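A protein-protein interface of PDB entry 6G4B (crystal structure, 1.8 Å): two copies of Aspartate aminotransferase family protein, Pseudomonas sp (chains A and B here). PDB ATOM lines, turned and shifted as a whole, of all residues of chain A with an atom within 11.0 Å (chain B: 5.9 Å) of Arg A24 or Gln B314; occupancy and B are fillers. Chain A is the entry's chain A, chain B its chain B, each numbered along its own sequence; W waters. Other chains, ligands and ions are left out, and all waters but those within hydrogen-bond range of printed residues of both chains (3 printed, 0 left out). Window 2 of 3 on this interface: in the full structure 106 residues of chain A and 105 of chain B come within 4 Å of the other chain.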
ATOM      1  N   ASP A  12       2.738 -23.751  17.728  1.00  0.00           N
ATOM      2  CA  ASP A  12       1.968 -23.255  18.842  1.00  0.00           C
ATOM      3  C   ASP A  12       0.745 -24.142  19.059  1.00  0.00           C
ATOM      4  O   ASP A  12       0.450 -24.533  20.181  1.00  0.00           O
ATOM      5  CB  ASP A  12       1.518 -21.830  18.593  1.00  0.00           C
ATOM      6  CG  ASP A  12       0.662 -21.300  19.712  1.00  0.00           C
ATOM      7  OD1 ASP A  12       1.226 -20.911  20.745  1.00  0.00           O
ATOM      8  OD2 ASP A  12      -0.577 -21.271  19.551  1.00  0.00           O
ATOM      9  N   ILE A  13       0.071 -24.477  17.956  1.00  0.00           N
ATOM     10  CA  ILE A  13      -1.093 -25.361  18.017  1.00  0.00           C
ATOM     11  C   ILE A  13      -0.721 -26.762  18.542  1.00  0.00           C
ATOM     12  O   ILE A  13      -1.467 -27.373  19.318  1.00  0.00           O
ATOM     13  CB  ILE A  13      -1.746 -25.492  16.620  1.00  0.00           C
ATOM     14  CG1 ILE A  13      -2.441 -24.165  16.276  1.00  0.00           C
ATOM     15  CG2 ILE A  13      -2.713 -26.664  16.578  1.00  0.00           C
ATOM     16  CD1 ILE A  13      -2.845 -24.086  14.823  1.00  0.00           C
ATOM     17  N   GLN A  14       0.427 -27.265  18.107  1.00  0.00           N
ATOM     18  CA  GLN A  14       0.865 -28.599  18.512  1.00  0.00           C
ATOM     19  C   GLN A  14       1.237 -28.697  19.990  1.00  0.00           C
ATOM     20  O   GLN A  14       1.001 -29.732  20.619  1.00  0.00           O
ATOM     21  CB  GLN A  14       2.063 -29.036  17.654  1.00  0.00           C
ATOM     22  CG  GLN A  14       2.474 -30.491  17.855  1.00  0.00           C
ATOM     23  CD  GLN A  14       1.384 -31.462  17.433  1.00  0.00           C
ATOM     24  OE1 GLN A  14       0.869 -31.373  16.307  1.00  0.00           O
ATOM     25  NE2 GLN A  14       1.012 -32.390  18.324  1.00  0.00           N
ATOM     26  N   GLN A  16       1.189 -25.873  22.762  1.00  0.00           N
ATOM     27  CA  GLN A  16       0.774 -24.984  23.859  1.00  0.00           C
ATOM     28  C   GLN A  16      -0.701 -25.050  24.192  1.00  0.00           C
ATOM     29  O   GLN A  16      -1.562 -24.956  23.309  1.00  0.00           O
ATOM     30  CB  GLN A  16       1.106 -23.543  23.541  1.00  0.00           C
ATOM     31  CG  GLN A  16       2.583 -23.288  23.370  1.00  0.00           C
ATOM     32  CD  GLN A  16       2.993 -21.940  23.930  1.00  0.00           C
ATOM     33  OE1 GLN A  16       3.265 -21.805  25.123  1.00  0.00           O
ATOM     34  NE2 GLN A  16       3.003 -20.934  23.082  1.00  0.00           N
ATOM     35  N   LEU A  17      -0.988 -25.212  25.472  1.00  0.00           N
ATOM     36  CA  LEU A  17      -2.346 -25.053  25.991  1.00  0.00           C
ATOM     37  C   LEU A  17      -2.508 -23.625  26.486  1.00  0.00           C
ATOM     38  O   LEU A  17      -1.861 -23.217  27.463  1.00  0.00           O
ATOM     39  CB  LEU A  17      -2.582 -26.030  27.139  1.00  0.00           C
ATOM     40  CG  LEU A  17      -3.911 -25.879  27.869  1.00  0.00           C
ATOM     41  CD1 LEU A  17      -5.053 -26.208  26.917  1.00  0.00           C
ATOM     42  CD2 LEU A  17      -3.953 -26.786  29.087  1.00  0.00           C
ATOM     43  N   HIS A  18      -3.346 -22.852  25.817  1.00  0.00           N
ATOM     44  CA  HIS A  18      -3.458 -21.431  26.109  1.00  0.00           C
ATOM     45  C   HIS A  18      -4.418 -21.120  27.252  1.00  0.00           C
ATOM     46  O   HIS A  18      -5.526 -21.642  27.291  1.00  0.00           O
ATOM     47  CB  HIS A  18      -3.874 -20.628  24.852  1.00  0.00           C
ATOM     48  CG  HIS A  18      -2.732 -20.383  23.914  1.00  0.00           C
ATOM     49  ND1 HIS A  18      -2.073 -19.171  23.846  1.00  0.00           N
ATOM     50  CD2 HIS A  18      -2.074 -21.219  23.075  1.00  0.00           C
ATOM     51  CE1 HIS A  18      -1.070 -19.269  22.988  1.00  0.00           C
ATOM     52  NE2 HIS A  18      -1.055 -20.493  22.496  1.00  0.00           N
ATOM     53  N   PRO A  19      -4.017 -20.206  28.143  1.00  0.00           N
ATOM     54  CA  PRO A  19      -4.988 -19.643  29.088  1.00  0.00           C
ATOM     55  C   PRO A  19      -6.109 -18.901  28.415  1.00  0.00           C
ATOM     56  O   PRO A  19      -5.908 -18.302  27.356  1.00  0.00           O
ATOM     57  CB  PRO A  19      -4.167 -18.639  29.906  1.00  0.00           C
ATOM     58  CG  PRO A  19      -2.752 -18.845  29.559  1.00  0.00           C
ATOM     59  CD  PRO A  19      -2.712 -19.531  28.215  1.00  0.00           C
ATOM     60  N   TYR A  20      -7.288 -18.916  29.042  1.00  0.00           N
ATOM     61  CA  TYR A  20      -8.402 -18.098  28.628  1.00  0.00           C
ATOM     62  C   TYR A  20      -8.669 -18.190  27.145  1.00  0.00           C
ATOM     63  O   TYR A  20      -8.935 -17.178  26.464  1.00  0.00           O
ATOM     64  CB  TYR A  20      -8.163 -16.652  29.080  1.00  0.00           C
ATOM     65  CG  TYR A  20      -8.245 -16.511  30.561  1.00  0.00           C
ATOM     66  CD1 TYR A  20      -9.484 -16.572  31.210  1.00  0.00           C
ATOM     67  CD2 TYR A  20      -7.100 -16.365  31.341  1.00  0.00           C
ATOM     68  CE1 TYR A  20      -9.579 -16.448  32.586  1.00  0.00           C
ATOM     69  CE2 TYR A  20      -7.179 -16.228  32.718  1.00  0.00           C
ATOM     70  CZ  TYR A  20      -8.410 -16.273  33.348  1.00  0.00           C
ATOM     71  OH  TYR A  20      -8.500 -16.126  34.732  1.00  0.00           O
ATOM     72  N   THR A  21      -8.650 -19.431  26.661  1.00  0.00           N
ATOM     73  CA  THR A  21      -8.822 -19.749  25.247  1.00  0.00           C
ATOM     74  C   THR A  21      -9.646 -21.023  25.139  1.00  0.00           C
ATOM     75  O   THR A  21      -9.503 -21.922  25.978  1.00  0.00           O
ATOM     76  CB  THR A  21      -7.442 -19.926  24.562  1.00  0.00           C
ATOM     77  OG1 THR A  21      -6.675 -18.720  24.744  1.00  0.00           O
ATOM     78  CG2 THR A  21      -7.583 -20.234  23.089  1.00  0.00           C
ATOM     79  N   ASN A  22     -10.498 -21.076  24.117  1.00  0.00           N
ATOM     80  CA  ASN A  22     -11.207 -22.294  23.700  1.00  0.00           C
ATOM     81  C   ASN A  22     -10.178 -23.150  22.962  1.00  0.00           C
ATOM     82  O   ASN A  22      -9.751 -22.802  21.852  1.00  0.00           O
ATOM     83  CB  ASN A  22     -12.389 -21.932  22.791  1.00  0.00           C
ATOM     84  CG  ASN A  22     -13.048 -23.146  22.135  1.00  0.00           C
ATOM     85  OD1 ASN A  22     -12.443 -24.228  22.007  1.00  0.00           O
ATOM     86  ND2 ASN A  22     -14.284 -22.946  21.639  1.00  0.00           N
ATOM     87  N   ALA A  23      -9.754 -24.245  23.594  1.00  0.00           N
ATOM     88  CA  ALA A  23      -8.620 -25.027  23.073  1.00  0.00           C
ATOM     89  C   ALA A  23      -8.923 -25.670  21.723  1.00  0.00           C
ATOM     90  O   ALA A  23      -8.015 -25.822  20.897  1.00  0.00           O
ATOM     91  CB  ALA A  23      -8.177 -26.076  24.080  1.00  0.00           C
ATOM     92  N   ARG A  24     -10.175 -26.064  21.492  1.00  0.00           N
ATOM     93  CA  ARG A  24     -10.551 -26.661  20.212  1.00  0.00           C
ATOM     94  C   ARG A  24     -10.561 -25.633  19.075  1.00  0.00           C
ATOM     95  O   ARG A  24     -10.062 -25.884  17.974  1.00  0.00           O
ATOM     96  CB  ARG A  24     -11.921 -27.332  20.318  1.00  0.00           C
ATOM     97  CG  ARG A  24     -11.935 -28.513  21.286  1.00  0.00           C
ATOM     98  CD  ARG A  24     -10.894 -29.551  20.874  1.00  0.00           C
ATOM     99  NE  ARG A  24     -11.119 -30.842  21.525  1.00  0.00           N
ATOM    100  CZ  ARG A  24     -10.200 -31.799  21.637  1.00  0.00           C
ATOM    101  NH1 ARG A  24      -8.980 -31.638  21.122  1.00  0.00           N
ATOM    102  NH2 ARG A  24     -10.519 -32.935  22.226  1.00  0.00           N
ATOM    103  N   LEU A  25     -11.139 -24.475  19.344  1.00  0.00           N
ATOM    104  CA  LEU A  25     -11.133 -23.390  18.362  1.00  0.00           C
ATOM    105  C   LEU A  25      -9.687 -22.990  18.079  1.00  0.00           C
ATOM    106  O   LEU A  25      -9.337 -22.648  16.951  1.00  0.00           O
ATOM    107  CB  LEU A  25     -11.921 -22.206  18.906  1.00  0.00           C
ATOM    108  CG  LEU A  25     -12.053 -20.985  17.990  1.00  0.00           C
ATOM    109  CD1 LEU A  25     -12.740 -21.353  16.685  1.00  0.00           C
ATOM    110  CD2 LEU A  25     -12.827 -19.893  18.714  1.00  0.00           C
ATOM    111  N   HIS A  26      -8.839 -23.043  19.101  1.00  0.00           N
ATOM    112  CA  HIS A  26      -7.436 -22.691  18.916  1.00  0.00           C
ATOM    113  C   HIS A  26      -6.743 -23.640  17.950  1.00  0.00           C
ATOM    114  O   HIS A  26      -5.906 -23.227  17.153  1.00  0.00           O
ATOM    115  CB  HIS A  26      -6.677 -22.659  20.260  1.00  0.00           C
ATOM    116  CG  HIS A  26      -5.303 -22.110  20.123  1.00  0.00           C
ATOM    117  ND1 HIS A  26      -5.065 -20.769  19.942  1.00  0.00           N
ATOM    118  CD2 HIS A  26      -4.092 -22.710  20.087  1.00  0.00           C
ATOM    119  CE1 HIS A  26      -3.763 -20.560  19.834  1.00  0.00           C
ATOM    120  NE2 HIS A  26      -3.154 -21.723  19.915  1.00  0.00           N
ATOM    121  N   GLN A  27      -7.081 -24.930  18.035  1.00  0.00           N
ATOM    122  CA  GLN A  27      -6.528 -25.910  17.111  1.00  0.00           C
ATOM    123  C   GLN A  27      -6.894 -25.626  15.660  1.00  0.00           C
ATOM    124  O   GLN A  27      -6.143 -25.981  14.755  1.00  0.00           O
ATOM    125  CB  GLN A  27      -6.956 -27.319  17.502  1.00  0.00           C
ATOM    126  CG  GLN A  27      -6.301 -27.783  18.797  1.00  0.00           C
ATOM    127  CD  GLN A  27      -6.763 -29.162  19.192  1.00  0.00           C
ATOM    128  OE1 GLN A  27      -7.966 -29.401  19.358  1.00  0.00           O
ATOM    129  NE2 GLN A  27      -5.826 -30.095  19.296  1.00  0.00           N
ATOM    130  N   GLU A  28      -8.043 -25.001  15.438  1.00  0.00           N
ATOM    131  CA  GLU A  28      -8.406 -24.594  14.079  1.00  0.00           C
ATOM    132  C   GLU A  28      -7.759 -23.271  13.681  1.00  0.00           C
ATOM    133  O   GLU A  28      -7.116 -23.188  12.628  1.00  0.00           O
ATOM    134  CB  GLU A  28      -9.911 -24.460  13.935  1.00  0.00           C
ATOM    135  CG  GLU A  28     -10.307 -24.204  12.488  1.00  0.00           C
ATOM    136  CD  GLU A  28     -11.646 -23.523  12.337  1.00  0.00           C
ATOM    137  OE1 GLU A  28     -12.443 -23.551  13.297  1.00  0.00           O
ATOM    138  OE2 GLU A  28     -11.905 -22.971  11.230  1.00  0.00           O
ATOM    139  N   LEU A  29      -7.954 -22.226  14.489  1.00  0.00           N
ATOM    140  CA  LEU A  29      -7.548 -20.868  14.083  1.00  0.00           C
ATOM    141  C   LEU A  29      -6.080 -20.587  14.300  1.00  0.00           C
ATOM    142  O   LEU A  29      -5.486 -19.765  13.595  1.00  0.00           O
ATOM    143  CB  LEU A  29      -8.327 -19.810  14.865  1.00  0.00           C
ATOM    144  CG  LEU A  29      -9.839 -19.877  14.773  1.00  0.00           C
ATOM    145  CD1 LEU A  29     -10.424 -18.729  15.586  1.00  0.00           C
ATOM    146  CD2 LEU A  29     -10.305 -19.855  13.323  1.00  0.00           C
ATOM    147  N   GLY A  30      -5.506 -21.225  15.318  1.00  0.00           N
ATOM    148  CA  GLY A  30      -4.145 -20.912  15.700  1.00  0.00           C
ATOM    149  C   GLY A  30      -4.017 -19.562  16.403  1.00  0.00           C
ATOM    150  O   GLY A  30      -5.001 -18.853  16.634  1.00  0.00           O
ATOM    151  N   PRO A  31      -2.782 -19.173  16.709  1.00  0.00           N
ATOM    152  CA  PRO A  31      -2.520 -17.985  17.493  1.00  0.00           C
ATOM    153  C   PRO A  31      -2.464 -16.710  16.671  1.00  0.00           C
ATOM    154  O   PRO A  31      -2.346 -16.756  15.442  1.00  0.00           O
ATOM    155  CB  PRO A  31      -1.133 -18.259  18.053  1.00  0.00           C
ATOM    156  CG  PRO A  31      -0.462 -19.061  16.972  1.00  0.00           C
ATOM    157  CD  PRO A  31      -1.550 -19.935  16.427  1.00  0.00           C
ATOM    158  N   ARG A 169     -16.661 -22.275  37.414  1.00  0.00           N
ATOM    159  CA  ARG A 169     -17.411 -23.329  36.762  1.00  0.00           C
ATOM    160  C   ARG A 169     -16.464 -24.375  36.187  1.00  0.00           C
ATOM    161  O   ARG A 169     -15.542 -24.041  35.472  1.00  0.00           O
ATOM    162  CB  ARG A 169     -18.262 -22.703  35.655  1.00  0.00           C
ATOM    163  CG  ARG A 169     -19.267 -23.607  34.985  1.00  0.00           C
ATOM    164  CD  ARG A 169     -20.052 -22.787  33.959  1.00  0.00           C
ATOM    165  NE  ARG A 169     -20.985 -23.630  33.226  1.00  0.00           N
ATOM    166  CZ  ARG A 169     -21.417 -23.400  31.980  1.00  0.00           C
ATOM    167  NH1 ARG A 169     -20.967 -22.356  31.274  1.00  0.00           N
ATOM    168  NH2 ARG A 169     -22.268 -24.248  31.424  1.00  0.00           N
ATOM    169  N   GLY A 170     -16.681 -25.634  36.533  1.00  0.00           N
ATOM    170  CA  GLY A 170     -15.829 -26.732  36.095  1.00  0.00           C
ATOM    171  C   GLY A 170     -14.661 -27.011  37.016  1.00  0.00           C
ATOM    172  O   GLY A 170     -14.026 -28.051  36.882  1.00  0.00           O
ATOM    173  N   PHE A 171     -14.377 -26.098  37.962  1.00  0.00           N
ATOM    174  CA  PHE A 171     -13.199 -26.208  38.852  1.00  0.00           C
ATOM    175  C   PHE A 171     -13.560 -26.564  40.306  1.00  0.00           C
ATOM    176  O   PHE A 171     -12.690 -26.581  41.180  1.00  0.00           O
ATOM    177  CB  PHE A 171     -12.414 -24.896  38.867  1.00  0.00           C
ATOM    178  CG  PHE A 171     -11.734 -24.577  37.574  1.00  0.00           C
ATOM    179  CD1 PHE A 171     -10.662 -25.340  37.127  1.00  0.00           C
ATOM    180  CD2 PHE A 171     -12.169 -23.508  36.789  1.00  0.00           C
ATOM    181  CE1 PHE A 171     -10.021 -25.021  35.942  1.00  0.00           C
ATOM    182  CE2 PHE A 171     -11.537 -23.192  35.603  1.00  0.00           C
ATOM    183  CZ  PHE A 171     -10.456 -23.950  35.174  1.00  0.00           C
ATOM    184  N   ARG A 403     -17.646  -9.836  22.293  1.00  0.00           N
ATOM    185  CA  ARG A 403     -16.742 -10.665  21.487  1.00  0.00           C
ATOM    186  C   ARG A 403     -16.573 -10.073  20.088  1.00  0.00           C
ATOM    187  O   ARG A 403     -15.450  -9.942  19.578  1.00  0.00           O
ATOM    188  CB  ARG A 403     -17.269 -12.088  21.406  1.00  0.00           C
ATOM    189  CG  ARG A 403     -16.363 -13.059  20.665  1.00  0.00           C
ATOM    190  CD  ARG A 403     -17.065 -14.410  20.419  1.00  0.00           C
ATOM    191  NE  ARG A 403     -16.120 -15.489  20.108  1.00  0.00           N
ATOM    192  CZ  ARG A 403     -15.553 -15.704  18.923  1.00  0.00           C
ATOM    193  NH1 ARG A 403     -14.739 -16.746  18.760  1.00  0.00           N
ATOM    194  NH2 ARG A 403     -15.788 -14.912  17.883  1.00  0.00           N
ATOM    195  N   TYR B 131     -10.986 -30.272  36.763  1.00  0.00           N
ATOM    196  CA  TYR B 131     -11.628 -29.843  35.518  1.00  0.00           C
ATOM    197  C   TYR B 131     -11.780 -31.035  34.568  1.00  0.00           C
ATOM    198  O   TYR B 131     -12.847 -31.265  34.005  1.00  0.00           O
ATOM    199  CB  TYR B 131     -10.777 -28.753  34.898  1.00  0.00           C
ATOM    200  CG  TYR B 131     -11.373 -27.894  33.810  1.00  0.00           C
ATOM    201  CD1 TYR B 131     -12.166 -26.786  34.111  1.00  0.00           C
ATOM    202  CD2 TYR B 131     -11.058 -28.120  32.476  1.00  0.00           C
ATOM    203  CE1 TYR B 131     -12.644 -25.941  33.125  1.00  0.00           C
ATOM    204  CE2 TYR B 131     -11.541 -27.286  31.473  1.00  0.00           C
ATOM    205  CZ  TYR B 131     -12.342 -26.191  31.792  1.00  0.00           C
ATOM    206  OH  TYR B 131     -12.809 -25.345  30.781  1.00  0.00           O
ATOM    207  N   PHE B 306      -4.951 -33.568  28.123  1.00  0.00           N
ATOM    208  CA  PHE B 306      -5.251 -32.454  27.220  1.00  0.00           C
ATOM    209  C   PHE B 306      -6.613 -32.583  26.565  1.00  0.00           C
ATOM    210  O   PHE B 306      -7.375 -31.614  26.479  1.00  0.00           O
ATOM    211  CB  PHE B 306      -4.207 -32.318  26.108  1.00  0.00           C
ATOM    212  CG  PHE B 306      -4.642 -31.395  25.016  1.00  0.00           C
ATOM    213  CD1 PHE B 306      -4.838 -30.038  25.278  1.00  0.00           C
ATOM    214  CD2 PHE B 306      -4.930 -31.881  23.751  1.00  0.00           C
ATOM    215  CE1 PHE B 306      -5.263 -29.168  24.283  1.00  0.00           C
ATOM    216  CE2 PHE B 306      -5.371 -31.012  22.750  1.00  0.00           C
ATOM    217  CZ  PHE B 306      -5.532 -29.664  23.019  1.00  0.00           C
ATOM    218  N   GLU B 307      -6.922 -33.760  26.044  1.00  0.00           N
ATOM    219  CA  GLU B 307      -8.152 -33.892  25.252  1.00  0.00           C
ATOM    220  C   GLU B 307      -9.409 -33.609  26.085  1.00  0.00           C
ATOM    221  O   GLU B 307     -10.334 -32.963  25.603  1.00  0.00           O
ATOM    222  CB  GLU B 307      -8.261 -35.283  24.620  1.00  0.00           C
ATOM    223  CG  GLU B 307      -7.165 -35.596  23.607  1.00  0.00           C
ATOM    224  CD  GLU B 307      -7.183 -34.742  22.355  1.00  0.00           C
ATOM    225  OE1 GLU B 307      -8.257 -34.295  21.916  1.00  0.00           O
ATOM    226  OE2 GLU B 307      -6.088 -34.540  21.780  1.00  0.00           O
ATOM    227  N   GLY B 308      -9.442 -34.096  27.321  1.00  0.00           N
ATOM    228  CA  GLY B 308     -10.570 -33.808  28.217  1.00  0.00           C
ATOM    229  C   GLY B 308     -10.699 -32.339  28.578  1.00  0.00           C
ATOM    230  O   GLY B 308     -11.792 -31.752  28.525  1.00  0.00           O
ATOM    231  N   ILE B 309      -9.575 -31.726  28.936  1.00  0.00           N
ATOM    232  CA  ILE B 309      -9.543 -30.297  29.228  1.00  0.00           C
ATOM    233  C   ILE B 309     -10.014 -29.513  28.005  1.00  0.00           C
ATOM    234  O   ILE B 309     -10.837 -28.596  28.114  1.00  0.00           O
ATOM    235  CB  ILE B 309      -8.122 -29.858  29.650  1.00  0.00           C
ATOM    236  CG1 ILE B 309      -7.787 -30.470  31.010  1.00  0.00           C
ATOM    237  CG2 ILE B 309      -8.005 -28.341  29.685  1.00  0.00           C
ATOM    238  CD1 ILE B 309      -6.361 -30.303  31.423  1.00  0.00           C
ATOM    239  N   ALA B 310      -9.516 -29.887  26.833  1.00  0.00           N
ATOM    240  CA  ALA B 310      -9.846 -29.169  25.611  1.00  0.00           C
ATOM    241  C   ALA B 310     -11.345 -29.209  25.322  1.00  0.00           C
ATOM    242  O   ALA B 310     -11.955 -28.192  24.991  1.00  0.00           O
ATOM    243  CB  ALA B 310      -9.035 -29.727  24.445  1.00  0.00           C
ATOM    244  N   ASP B 311     -11.940 -30.389  25.444  1.00  0.00           N
ATOM    245  CA  ASP B 311     -13.381 -30.556  25.238  1.00  0.00           C
ATOM    246  C   ASP B 311     -14.196 -29.663  26.142  1.00  0.00           C
ATOM    247  O   ASP B 311     -15.133 -28.990  25.697  1.00  0.00           O
ATOM    248  CB  ASP B 311     -13.803 -32.004  25.486  1.00  0.00           C
ATOM    249  CG  ASP B 311     -13.517 -32.911  24.310  1.00  0.00           C
ATOM    250  OD1 ASP B 311     -13.143 -32.420  23.204  1.00  0.00           O
ATOM    251  OD2 ASP B 311     -13.680 -34.138  24.480  1.00  0.00           O
ATOM    252  N   GLN B 312     -13.842 -29.640  27.415  1.00  0.00           N
ATOM    253  CA  GLN B 312     -14.600 -28.844  28.355  1.00  0.00           C
ATOM    254  C   GLN B 312     -14.399 -27.347  28.105  1.00  0.00           C
ATOM    255  O   GLN B 312     -15.343 -26.575  28.266  1.00  0.00           O
ATOM    256  CB  GLN B 312     -14.237 -29.205  29.785  1.00  0.00           C
ATOM    257  CG  GLN B 312     -15.252 -28.556  30.750  1.00  0.00           C
ATOM    258  CD  GLN B 312     -15.322 -29.202  32.117  1.00  0.00           C
ATOM    259  OE1 GLN B 312     -14.444 -28.981  32.973  1.00  0.00           O
ATOM    260  NE2 GLN B 312     -16.361 -29.948  32.359  1.00  0.00           N
ATOM    261  N   SER B 313     -13.184 -26.940  27.710  1.00  0.00           N
ATOM    262  CA  SER B 313     -12.908 -25.520  27.421  1.00  0.00           C
ATOM    263  C   SER B 313     -13.805 -25.018  26.281  1.00  0.00           C
ATOM    264  O   SER B 313     -14.154 -23.830  26.221  1.00  0.00           O
ATOM    265  CB  SER B 313     -11.439 -25.298  27.082  1.00  0.00           C
ATOM    266  OG  SER B 313     -11.115 -25.736  25.773  1.00  0.00           O
ATOM    267  N   GLN B 314     -14.149 -25.927  25.376  1.00  0.00           N
ATOM    268  CA  GLN B 314     -15.048 -25.621  24.292  1.00  0.00           C
ATOM    269  C   GLN B 314     -16.487 -25.468  24.807  1.00  0.00           C
ATOM    270  O   GLN B 314     -17.150 -24.481  24.518  1.00  0.00           O
ATOM    271  CB  GLN B 314     -14.942 -26.742  23.265  1.00  0.00           C
ATOM    272  CG  GLN B 314     -15.903 -26.715  22.118  1.00  0.00           C
ATOM    273  CD  GLN B 314     -15.601 -27.873  21.174  1.00  0.00           C
ATOM    274  OE1 GLN B 314     -15.678 -29.037  21.570  1.00  0.00           O
ATOM    275  NE2 GLN B 314     -15.261 -27.566  19.941  1.00  0.00           N
ATOM    276  N   ALA B 315     -16.953 -26.456  25.559  1.00  0.00           N
ATOM    277  CA  ALA B 315     -18.329 -26.438  26.087  1.00  0.00           C
ATOM    278  C   ALA B 315     -18.580 -25.230  26.982  1.00  0.00           C
ATOM    279  O   ALA B 315     -19.684 -24.666  26.994  1.00  0.00           O
ATOM    280  CB  ALA B 315     -18.590 -27.718  26.861  1.00  0.00           C
ATOM    281  N   LEU B 316     -17.561 -24.840  27.743  1.00  0.00           N
ATOM    282  CA  LEU B 316     -17.656 -23.683  28.644  1.00  0.00           C
ATOM    283  C   LEU B 316     -17.133 -22.367  28.078  1.00  0.00           C
ATOM    284  O   LEU B 316     -16.944 -21.421  28.844  1.00  0.00           O
ATOM    285  CB  LEU B 316     -16.938 -23.978  29.971  1.00  0.00           C
ATOM    286  CG  LEU B 316     -17.318 -25.258  30.715  1.00  0.00           C
ATOM    287  CD1 LEU B 316     -16.505 -25.332  32.014  1.00  0.00           C
ATOM    288  CD2 LEU B 316     -18.815 -25.343  30.994  1.00  0.00           C
ATOM    289  N   GLY B 317     -16.830 -22.305  26.781  1.00  0.00           N
ATOM    290  CA  GLY B 317     -16.473 -21.040  26.140  1.00  0.00           C
ATOM    291  C   GLY B 317     -14.983 -20.798  26.033  1.00  0.00           C
ATOM    292  O   GLY B 317     -14.480 -20.488  24.963  1.00  0.00           O
ATOM    293  N   ALA B 318     -14.279 -20.915  27.153  1.00  0.00           N
ATOM    294  CA  ALA B 318     -12.816 -20.833  27.181  1.00  0.00           C
ATOM    295  C   ALA B 318     -12.336 -21.471  28.470  1.00  0.00           C
ATOM    296  O   ALA B 318     -13.125 -21.655  29.394  1.00  0.00           O
ATOM    297  CB  ALA B 318     -12.347 -19.388  27.087  1.00  0.00           C
HETATM  298  O   HOH W   1     -15.322 -24.840  19.586  1.00  0.00           O
HETATM  299  O   HOH W   2      -5.916 -32.978  19.769  1.00  0.00           O
HETATM  300  O   HOH W   3     -21.398 -23.105  28.062  1.00  0.00           O
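The backbone NH (N) of Ala A23 lies within hydrogen-bond range of the side-chain hydroxyl (OG) of Ser B313, at 3.0 Å.
NH2 of Arg A24 is in salt-bridge range of OE1 of Glu B307 (2.7 Å).
The side-chain carboxylate (OD1) of Asp B311 lies within salt-bridge range of the guanidinium group (NH2) of Arg A24 (2.8 Å).
OG1 of Thr A21 lies within hydrogen-bond range of O of Pro A19, 2.8 Å away.
The side-chain amide oxygen of Asn A22 lies within hydrogen-bond range of the backbone NH of Arg A24 (3.0 Å).
The guanidinium group (NH1) of Arg A24 is in hydrogen-bond range of the side-chain amide oxygen (OE1) of Gln A27, at 3.0 Å.
The backbone carbonyl oxygen (O) of Tyr B131 sits close to the side-chain amide oxygen (OE1) of Gln B312 (3.0 Å).
N of Ser B313 sits close to OH of Tyr B131 (3.5 Å).
The backbone carbonyl oxygen (O) of Ala B310 lies within hydrogen-bond range of the side-chain hydroxyl (OG) of Ser B313 (2.7 Å).
CB of Ala B318 touches C of Tyr A20 (3.9 Å).
Ser B313 touches Asn A22 (OG to C, 3.9 Å).
Gly B317 touches Asn A22 (O to CB, 3.3 Å).
CA of Ala B318 touches N of Asn A22, 3.8 Å away.
Ala A23 touches Ala B310 (CB to CB, 3.8 Å).
Ala B310 touches Arg A24 (CB to CZ, 3.7 Å).
Gln B314 touches Arg A24.
CD2 of Leu B316 touches CZ of Arg A169, at 3.4 Å.
Gly A170 touches Tyr B131.
CD1 of Tyr B131 touches CE1 of Phe A171 (3.3 Å).
Printed residues of chain B within 4 Å of Arg A24: Glu B307, Ala B310, Asp B311 and Gln B314.
Of the printed residues of chain B, Gln A27 touches Phe B306.
Of the printed residues of chain B, Phe A171 touches Tyr B131 (3.3 Å).
Printed residues of chain A within 4 Å of Tyr B131: Gly A170 (3.3 Å) and Phe A171 (3.3 Å).
Printed residues of chain A within 4 Å of Phe B306: Leu A17 (3.97 Å) and Gln A27 (3.6 Å).
Glu B307 touches just one residue of chain A: Arg A24 (2.7 Å).
Ala B310 touches just these residues of chain A: Ala A23 (3.8 Å) and Arg A24 (3.7 Å).
Asp B311 touches just one residue of chain A: Arg A24 (2.8 Å).
Ser B313 touches two residues of chain A.
Gln B314 touches just these residues of chain A: Asn A22 (3.7 Å) and Arg A24 (3.4 Å).
Of the printed residues of chain A, Leu B316 touches Arg A169.
The nearest printed residue of chain A that does not touch Leu B316 is Gly A170 (4.4 Å).
Of the 14 printed residues of chain B, 10 touch a printed residue of chain A.
Hydrophobic or aromatic side chains of chain A within 4 Å of the printed part of chain B: Leu A17, Ala A23 and Phe A171.
Along chain A the printed residues that touch a printed residue of chain B span positions 17 to 171.
No position is printed for both chains.
Water W2 bridges OE2 of Glu B307 (2.6 Å) and NE2 of Gln A27 (2.9 Å).
Water W3 lies within hydrogen-bond range of the backbone carbonyl oxygen (O) of Ala B315 and the guanidinium group (NH1) of Arg A169.
Water W1 bridges NE2 of Gln B314 (2.7 Å) and ND2 of Asn A22 (3.0 Å).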
